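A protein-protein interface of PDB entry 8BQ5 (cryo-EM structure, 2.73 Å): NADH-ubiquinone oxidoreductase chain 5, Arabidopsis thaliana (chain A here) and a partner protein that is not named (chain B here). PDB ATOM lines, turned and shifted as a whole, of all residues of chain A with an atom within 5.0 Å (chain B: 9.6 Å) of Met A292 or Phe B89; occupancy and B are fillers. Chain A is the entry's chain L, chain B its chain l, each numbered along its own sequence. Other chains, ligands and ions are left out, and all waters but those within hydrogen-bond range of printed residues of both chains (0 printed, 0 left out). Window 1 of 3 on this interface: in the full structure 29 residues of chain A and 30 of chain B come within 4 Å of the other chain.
No residue of chain B comes within 4 Å of Ala A289. No residue of chain B comes within 4 Å of Gly A290. No residue of chain B comes within 4 Å of Ala A291. Met A292 touches one residue of chain B. No residue of chain B comes within 4 Å of Ser A294. Printed residues of chain B within 4 Å of Phe A418: Phe B89 (3.6 Å), Leu B92 (3.98 Å) and Gly B93 (3.9 Å). Printed residues of chain B within 4 Å of Leu A422: Phe B89 (3.9 Å) and Leu B92 (3.7 Å). Of the printed residues of chain A, Phe B89 touches Met A292 (3.6 Å), Phe A295 (3.6 Å), Phe A418 (3.6 Å), Leu A422 (3.9 Å) and Trp A563 (3.8 Å). Printed residues of chain A within 4 Å of Gly B93: Phe A418 (3.9 Å). The nearest residue of chain B that does not touch Met A292 is Leu B86 (6.0 Å). The nearest printed residue of chain A that does not touch Phe B88 is Leu A422 (4.1 Å).
Phe B88 touches Phe A295 (CE2 to CE2, 3.5 Å). Phe B89 touches Phe A295. O of Phe B89 touches CE1 of Phe A418, at 3.6 Å. CB of Leu B92 touches CE1 of Phe A418, at 3.98 Å. Phe A418 touches Gly B93. CE1 of Phe B89 touches CD1 of Leu A422, 3.9 Å away. Leu A422 touches Leu B92 (CD2 to CD2, 3.7 Å). O of Trp A563 touches CD1 of Leu B82, 3.3 Å away. CA of Gly B85 touches CZ3 of Trp A563, at 3.6 Å. CZ of Phe B89 touches CH2 of Trp A563, 3.8 Å away.
Of the 16 printed residues of chain B, 6 touch a printed residue of chain A. Hydrophobic or aromatic side chains of chain B within 4 Å of the printed part of chain A: Leu B82, Phe B88, Phe B89 and Leu B92. Of the 13 printed residues of chain A, 5 touch a printed residue of chain B. Hydrophobic or aromatic side chains of chain A that line the printed part of chain B: Met A292, Phe A295, Phe A418, Leu A422 and Trp A563.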
ATOM      1  N   ILE A 236      -8.788 -11.634 -20.468  1.00  0.00           N
ATOM      2  CA  ILE A 236      -8.415 -11.213 -19.118  1.00  0.00           C
ATOM      3  C   ILE A 236      -9.299 -11.810 -18.026  1.00  0.00           C
ATOM      4  O   ILE A 236      -8.793 -12.292 -17.005  1.00  0.00           O
ATOM      5  CB  ILE A 236      -8.412  -9.672 -19.041  1.00  0.00           C
ATOM      6  CG1 ILE A 236      -8.132  -9.185 -17.618  1.00  0.00           C
ATOM      7  CG2 ILE A 236      -9.707  -9.091 -19.590  1.00  0.00           C
ATOM      8  CD1 ILE A 236      -6.753  -9.499 -17.129  1.00  0.00           C
ATOM      9  N   PHE A 288      -9.882  -2.484 -24.448  1.00  0.00           N
ATOM     10  CA  PHE A 288      -9.190  -2.555 -23.166  1.00  0.00           C
ATOM     11  C   PHE A 288      -8.878  -3.996 -22.781  1.00  0.00           C
ATOM     12  O   PHE A 288      -7.775  -4.294 -22.309  1.00  0.00           O
ATOM     13  CB  PHE A 288     -10.027  -1.885 -22.076  1.00  0.00           C
ATOM     14  CG  PHE A 288      -9.790  -0.407 -21.947  1.00  0.00           C
ATOM     15  CD1 PHE A 288      -8.545   0.078 -21.590  1.00  0.00           C
ATOM     16  CD2 PHE A 288     -10.819   0.494 -22.152  1.00  0.00           C
ATOM     17  CE1 PHE A 288      -8.324   1.435 -21.465  1.00  0.00           C
ATOM     18  CE2 PHE A 288     -10.604   1.852 -22.024  1.00  0.00           C
ATOM     19  CZ  PHE A 288      -9.355   2.322 -21.680  1.00  0.00           C
ATOM     20  N   ALA A 289      -9.841  -4.902 -22.969  1.00  0.00           N
ATOM     21  CA  ALA A 289      -9.657  -6.286 -22.544  1.00  0.00           C
ATOM     22  C   ALA A 289      -8.588  -6.984 -23.376  1.00  0.00           C
ATOM     23  O   ALA A 289      -7.759  -7.731 -22.843  1.00  0.00           O
ATOM     24  CB  ALA A 289     -10.983  -7.040 -22.624  1.00  0.00           C
ATOM     25  N   GLY A 290      -8.598  -6.759 -24.691  1.00  0.00           N
ATOM     26  CA  GLY A 290      -7.615  -7.404 -25.545  1.00  0.00           C
ATOM     27  C   GLY A 290      -6.192  -6.994 -25.220  1.00  0.00           C
ATOM     28  O   GLY A 290      -5.298  -7.839 -25.131  1.00  0.00           O
ATOM     29  N   ALA A 291      -5.961  -5.692 -25.037  1.00  0.00           N
ATOM     30  CA  ALA A 291      -4.616  -5.212 -24.734  1.00  0.00           C
ATOM     31  C   ALA A 291      -4.145  -5.710 -23.374  1.00  0.00           C
ATOM     32  O   ALA A 291      -2.974  -6.061 -23.199  1.00  0.00           O
ATOM     33  CB  ALA A 291      -4.579  -3.686 -24.790  1.00  0.00           C
ATOM     34  N   MET A 292      -5.049  -5.736 -22.392  1.00  0.00           N
ATOM     35  CA  MET A 292      -4.683  -6.199 -21.057  1.00  0.00           C
ATOM     36  C   MET A 292      -4.260  -7.662 -21.074  1.00  0.00           C
ATOM     37  O   MET A 292      -3.301  -8.046 -20.396  1.00  0.00           O
ATOM     38  CB  MET A 292      -5.850  -5.988 -20.095  1.00  0.00           C
ATOM     39  CG  MET A 292      -5.756  -4.712 -19.284  1.00  0.00           C
ATOM     40  SD  MET A 292      -6.995  -4.626 -17.981  1.00  0.00           S
ATOM     41  CE  MET A 292      -8.498  -4.609 -18.951  1.00  0.00           C
ATOM     42  N   THR A 293      -4.972  -8.493 -21.838  1.00  0.00           N
ATOM     43  CA  THR A 293      -4.665  -9.919 -21.882  1.00  0.00           C
ATOM     44  C   THR A 293      -3.297 -10.178 -22.503  1.00  0.00           C
ATOM     45  O   THR A 293      -2.548 -11.042 -22.033  1.00  0.00           O
ATOM     46  CB  THR A 293      -5.758 -10.661 -22.652  1.00  0.00           C
ATOM     47  OG1 THR A 293      -7.006 -10.514 -21.966  1.00  0.00           O
ATOM     48  CG2 THR A 293      -5.431 -12.139 -22.766  1.00  0.00           C
ATOM     49  N   SER A 294      -2.953  -9.440 -23.562  1.00  0.00           N
ATOM     50  CA  SER A 294      -1.676  -9.657 -24.233  1.00  0.00           C
ATOM     51  C   SER A 294      -0.505  -9.407 -23.291  1.00  0.00           C
ATOM     52  O   SER A 294       0.455 -10.184 -23.261  1.00  0.00           O
ATOM     53  CB  SER A 294      -1.571  -8.758 -25.464  1.00  0.00           C
ATOM     54  OG  SER A 294      -1.351  -7.413 -25.085  1.00  0.00           O
ATOM     55  N   PHE A 295      -0.566  -8.323 -22.516  1.00  0.00           N
ATOM     56  CA  PHE A 295       0.478  -8.062 -21.532  1.00  0.00           C
ATOM     57  C   PHE A 295       0.484  -9.125 -20.442  1.00  0.00           C
ATOM     58  O   PHE A 295       1.552  -9.558 -19.996  1.00  0.00           O
ATOM     59  CB  PHE A 295       0.289  -6.674 -20.925  1.00  0.00           C
ATOM     60  CG  PHE A 295       1.369  -6.287 -19.962  1.00  0.00           C
ATOM     61  CD1 PHE A 295       2.600  -5.855 -20.423  1.00  0.00           C
ATOM     62  CD2 PHE A 295       1.158  -6.362 -18.597  1.00  0.00           C
ATOM     63  CE1 PHE A 295       3.597  -5.501 -19.540  1.00  0.00           C
ATOM     64  CE2 PHE A 295       2.153  -6.009 -17.709  1.00  0.00           C
ATOM     65  CZ  PHE A 295       3.373  -5.578 -18.182  1.00  0.00           C
ATOM     66  N   LEU A 296      -0.702  -9.556 -20.007  1.00  0.00           N
ATOM     67  CA  LEU A 296      -0.809 -10.563 -18.957  1.00  0.00           C
ATOM     68  C   LEU A 296      -0.098 -11.853 -19.341  1.00  0.00           C
ATOM     69  O   LEU A 296       0.733 -12.372 -18.587  1.00  0.00           O
ATOM     70  CB  LEU A 296      -2.281 -10.854 -18.671  1.00  0.00           C
ATOM     71  CG  LEU A 296      -2.594 -11.440 -17.299  1.00  0.00           C
ATOM     72  CD1 LEU A 296      -2.110 -10.505 -16.224  1.00  0.00           C
ATOM     73  CD2 LEU A 296      -4.072 -11.723 -17.151  1.00  0.00           C
ATOM     74  N   PHE A 418      -4.044   3.241 -25.102  1.00  0.00           N
ATOM     75  CA  PHE A 418      -3.811   2.184 -24.124  1.00  0.00           C
ATOM     76  C   PHE A 418      -3.295   0.917 -24.795  1.00  0.00           C
ATOM     77  O   PHE A 418      -2.330   0.300 -24.329  1.00  0.00           O
ATOM     78  CB  PHE A 418      -5.108   1.907 -23.366  1.00  0.00           C
ATOM     79  CG  PHE A 418      -4.990   0.846 -22.313  1.00  0.00           C
ATOM     80  CD1 PHE A 418      -4.476   1.143 -21.065  1.00  0.00           C
ATOM     81  CD2 PHE A 418      -5.411  -0.448 -22.571  1.00  0.00           C
ATOM     82  CE1 PHE A 418      -4.377   0.167 -20.093  1.00  0.00           C
ATOM     83  CE2 PHE A 418      -5.315  -1.427 -21.604  1.00  0.00           C
ATOM     84  CZ  PHE A 418      -4.799  -1.119 -20.364  1.00  0.00           C
ATOM     85  N   LEU A 422       0.510  -1.199 -24.526  1.00  0.00           N
ATOM     86  CA  LEU A 422       0.551  -2.569 -24.023  1.00  0.00           C
ATOM     87  C   LEU A 422       0.904  -3.556 -25.125  1.00  0.00           C
ATOM     88  O   LEU A 422       1.625  -4.531 -24.883  1.00  0.00           O
ATOM     89  CB  LEU A 422      -0.786  -2.932 -23.385  1.00  0.00           C
ATOM     90  CG  LEU A 422      -0.960  -2.484 -21.935  1.00  0.00           C
ATOM     91  CD1 LEU A 422      -2.128  -3.210 -21.301  1.00  0.00           C
ATOM     92  CD2 LEU A 422       0.314  -2.714 -21.141  1.00  0.00           C
ATOM     93  N   TRP A 563       0.312 -14.234 -11.757  1.00  0.00           N
ATOM     94  CA  TRP A 563      -0.193 -13.082 -11.014  1.00  0.00           C
ATOM     95  C   TRP A 563      -1.094 -13.475  -9.848  1.00  0.00           C
ATOM     96  O   TRP A 563      -1.868 -12.641  -9.367  1.00  0.00           O
ATOM     97  CB  TRP A 563      -0.948 -12.110 -11.933  1.00  0.00           C
ATOM     98  CG  TRP A 563      -0.107 -11.465 -12.993  1.00  0.00           C
ATOM     99  CD1 TRP A 563       0.923 -12.029 -13.687  1.00  0.00           C
ATOM    100  CD2 TRP A 563      -0.225 -10.122 -13.476  1.00  0.00           C
ATOM    101  NE1 TRP A 563       1.450 -11.124 -14.575  1.00  0.00           N
ATOM    102  CE2 TRP A 563       0.763  -9.945 -14.466  1.00  0.00           C
ATOM    103  CE3 TRP A 563      -1.075  -9.055 -13.174  1.00  0.00           C
ATOM    104  CZ2 TRP A 563       0.925  -8.744 -15.151  1.00  0.00           C
ATOM    105  CZ3 TRP A 563      -0.913  -7.865 -13.854  1.00  0.00           C
ATOM    106  CH2 TRP A 563       0.080  -7.718 -14.831  1.00  0.00           C
ATOM    107  N   LEU B  82      -2.126  -9.181  -6.402  1.00  0.00           N
ATOM    108  CA  LEU B  82      -2.915  -9.155  -7.630  1.00  0.00           C
ATOM    109  C   LEU B  82      -3.580  -7.800  -7.838  1.00  0.00           C
ATOM    110  O   LEU B  82      -3.763  -7.360  -8.979  1.00  0.00           O
ATOM    111  CB  LEU B  82      -3.961 -10.271  -7.606  1.00  0.00           C
ATOM    112  CG  LEU B  82      -4.966 -10.301  -8.761  1.00  0.00           C
ATOM    113  CD1 LEU B  82      -4.266 -10.554 -10.084  1.00  0.00           C
ATOM    114  CD2 LEU B  82      -6.024 -11.359  -8.514  1.00  0.00           C
ATOM    115  N   SER B  83      -3.961  -7.129  -6.750  1.00  0.00           N
ATOM    116  CA  SER B  83      -4.524  -5.789  -6.876  1.00  0.00           C
ATOM    117  C   SER B  83      -3.473  -4.799  -7.355  1.00  0.00           C
ATOM    118  O   SER B  83      -3.789  -3.845  -8.076  1.00  0.00           O
ATOM    119  CB  SER B  83      -5.123  -5.344  -5.545  1.00  0.00           C
ATOM    120  OG  SER B  83      -6.467  -5.778  -5.428  1.00  0.00           O
ATOM    121  N   GLY B  84      -2.215  -5.006  -6.961  1.00  0.00           N
ATOM    122  CA  GLY B  84      -1.142  -4.185  -7.495  1.00  0.00           C
ATOM    123  C   GLY B  84      -0.975  -4.351  -8.993  1.00  0.00           C
ATOM    124  O   GLY B  84      -0.758  -3.376  -9.714  1.00  0.00           O
ATOM    125  N   GLY B  85      -1.070  -5.591  -9.480  1.00  0.00           N
ATOM    126  CA  GLY B  85      -1.006  -5.815 -10.915  1.00  0.00           C
ATOM    127  C   GLY B  85      -2.181  -5.202 -11.650  1.00  0.00           C
ATOM    128  O   GLY B  85      -2.021  -4.623 -12.727  1.00  0.00           O
ATOM    129  N   LEU B  86      -3.382  -5.326 -11.082  1.00  0.00           N
ATOM    130  CA  LEU B  86      -4.535  -4.646 -11.657  1.00  0.00           C
ATOM    131  C   LEU B  86      -4.436  -3.139 -11.470  1.00  0.00           C
ATOM    132  O   LEU B  86      -5.069  -2.379 -12.210  1.00  0.00           O
ATOM    133  CB  LEU B  86      -5.822  -5.188 -11.038  1.00  0.00           C
ATOM    134  CG  LEU B  86      -6.130  -6.665 -11.311  1.00  0.00           C
ATOM    135  CD1 LEU B  86      -7.610  -6.947 -11.130  1.00  0.00           C
ATOM    136  CD2 LEU B  86      -5.681  -7.069 -12.708  1.00  0.00           C
ATOM    137  N   GLY B  87      -3.652  -2.691 -10.487  1.00  0.00           N
ATOM    138  CA  GLY B  87      -3.382  -1.272 -10.355  1.00  0.00           C
ATOM    139  C   GLY B  87      -2.448  -0.750 -11.427  1.00  0.00           C
ATOM    140  O   GLY B  87      -2.491   0.436 -11.767  1.00  0.00           O
ATOM    141  N   PHE B  88      -1.592  -1.616 -11.970  1.00  0.00           N
ATOM    142  CA  PHE B  88      -0.773  -1.222 -13.112  1.00  0.00           C
ATOM    143  C   PHE B  88      -1.647  -0.906 -14.318  1.00  0.00           C
ATOM    144  O   PHE B  88      -1.412   0.075 -15.032  1.00  0.00           O
ATOM    145  CB  PHE B  88       0.230  -2.323 -13.452  1.00  0.00           C
ATOM    146  CG  PHE B  88       0.863  -2.159 -14.803  1.00  0.00           C
ATOM    147  CD1 PHE B  88       1.841  -1.202 -15.010  1.00  0.00           C
ATOM    148  CD2 PHE B  88       0.470  -2.951 -15.869  1.00  0.00           C
ATOM    149  CE1 PHE B  88       2.422  -1.042 -16.254  1.00  0.00           C
ATOM    150  CE2 PHE B  88       1.045  -2.796 -17.113  1.00  0.00           C
ATOM    151  CZ  PHE B  88       2.023  -1.840 -17.307  1.00  0.00           C
ATOM    152  N   PHE B  89      -2.663  -1.737 -14.562  1.00  0.00           N
ATOM    153  CA  PHE B  89      -3.549  -1.514 -15.700  1.00  0.00           C
ATOM    154  C   PHE B  89      -4.376  -0.248 -15.513  1.00  0.00           C
ATOM    155  O   PHE B  89      -4.636   0.481 -16.477  1.00  0.00           O
ATOM    156  CB  PHE B  89      -4.460  -2.724 -15.900  1.00  0.00           C
ATOM    157  CG  PHE B  89      -3.741  -3.952 -16.382  1.00  0.00           C
ATOM    158  CD1 PHE B  89      -2.738  -3.858 -17.328  1.00  0.00           C
ATOM    159  CD2 PHE B  89      -4.080  -5.203 -15.894  1.00  0.00           C
ATOM    160  CE1 PHE B  89      -2.079  -4.985 -17.776  1.00  0.00           C
ATOM    161  CE2 PHE B  89      -3.424  -6.335 -16.337  1.00  0.00           C
ATOM    162  CZ  PHE B  89      -2.424  -6.225 -17.280  1.00  0.00           C
ATOM    163  N   VAL B  90      -4.812   0.019 -14.281  1.00  0.00           N
ATOM    164  CA  VAL B  90      -5.570   1.235 -14.003  1.00  0.00           C
ATOM    165  C   VAL B  90      -4.678   2.463 -14.133  1.00  0.00           C
ATOM    166  O   VAL B  90      -5.091   3.493 -14.677  1.00  0.00           O
ATOM    167  CB  VAL B  90      -6.225   1.145 -12.612  1.00  0.00           C
ATOM    168  CG1 VAL B  90      -6.516   2.532 -12.059  1.00  0.00           C
ATOM    169  CG2 VAL B  90      -7.502   0.336 -12.694  1.00  0.00           C
ATOM    170  N   GLY B  91      -3.441   2.373 -13.639  1.00  0.00           N
ATOM    171  CA  GLY B  91      -2.529   3.501 -13.748  1.00  0.00           C
ATOM    172  C   GLY B  91      -2.232   3.879 -15.186  1.00  0.00           C
ATOM    173  O   GLY B  91      -2.218   5.060 -15.538  1.00  0.00           O
ATOM    174  N   LEU B  92      -1.997   2.877 -16.039  1.00  0.00           N
ATOM    175  CA  LEU B  92      -1.752   3.140 -17.452  1.00  0.00           C
ATOM    176  C   LEU B  92      -2.981   3.734 -18.127  1.00  0.00           C
ATOM    177  O   LEU B  92      -2.859   4.576 -19.024  1.00  0.00           O
ATOM    178  CB  LEU B  92      -1.332   1.852 -18.158  1.00  0.00           C
ATOM    179  CG  LEU B  92      -0.379   1.993 -19.342  1.00  0.00           C
ATOM    180  CD1 LEU B  92       1.030   2.272 -18.851  1.00  0.00           C
ATOM    181  CD2 LEU B  92      -0.420   0.741 -20.201  1.00  0.00           C
ATOM    182  N   GLY B  93      -4.174   3.287 -17.728  1.00  0.00           N
ATOM    183  CA  GLY B  93      -5.388   3.863 -18.280  1.00  0.00           C
ATOM    184  C   GLY B  93      -5.516   5.342 -17.976  1.00  0.00           C
ATOM    185  O   GLY B  93      -5.948   6.126 -18.825  1.00  0.00           O
ATOM    186  N   LEU B  94      -5.148   5.744 -16.756  1.00  0.00           N
ATOM    187  CA  LEU B  94      -5.172   7.159 -16.399  1.00  0.00           C
ATOM    188  C   LEU B  94      -4.137   7.951 -17.187  1.00  0.00           C
ATOM    189  O   LEU B  94      -4.405   9.081 -17.610  1.00  0.00           O
ATOM    190  CB  LEU B  94      -4.945   7.326 -14.899  1.00  0.00           C
ATOM    191  CG  LEU B  94      -6.069   6.814 -13.999  1.00  0.00           C
ATOM    192  CD1 LEU B  94      -5.560   6.589 -12.588  1.00  0.00           C
ATOM    193  CD2 LEU B  94      -7.233   7.787 -14.000  1.00  0.00           C
ATOM    194  N   LEU B  95      -2.944   7.385 -17.382  1.00  0.00           N
ATOM    195  CA  LEU B  95      -1.944   8.052 -18.209  1.00  0.00           C
ATOM    196  C   LEU B  95      -2.453   8.243 -19.631  1.00  0.00           C
ATOM    197  O   LEU B  95      -2.160   9.257 -20.274  1.00  0.00           O
ATOM    198  CB  LEU B  95      -0.641   7.258 -18.214  1.00  0.00           C
ATOM    199  CG  LEU B  95       0.414   7.641 -17.177  1.00  0.00           C
ATOM    200  CD1 LEU B  95       1.412   6.509 -17.010  1.00  0.00           C
ATOM    201  CD2 LEU B  95       1.118   8.924 -17.581  1.00  0.00           C
ATOM    202  N   ALA B  96      -3.207   7.268 -20.143  1.00  0.00           N
ATOM    203  CA  ALA B  96      -3.846   7.435 -21.442  1.00  0.00           C
ATOM    204  C   ALA B  96      -4.888   8.546 -21.400  1.00  0.00           C
ATOM    205  O   ALA B  96      -5.145   9.204 -22.415  1.00  0.00           O
ATOM    206  CB  ALA B  96      -4.481   6.119 -21.890  1.00  0.00           C
ATOM    207  N   VAL B  97      -5.515   8.751 -20.240  1.00  0.00           N
ATOM    208  CA  VAL B  97      -6.444   9.865 -20.081  1.00  0.00           C
ATOM    209  C   VAL B  97      -5.684  11.187 -20.103  1.00  0.00           C
ATOM    210  O   VAL B  97      -6.074  12.140 -20.788  1.00  0.00           O
ATOM    211  CB  VAL B  97      -7.257   9.705 -18.783  1.00  0.00           C
ATOM    212  CG1 VAL B  97      -7.746  11.056 -18.285  1.00  0.00           C
ATOM    213  CG2 VAL B  97      -8.418   8.747 -18.989  1.00  0.00           C
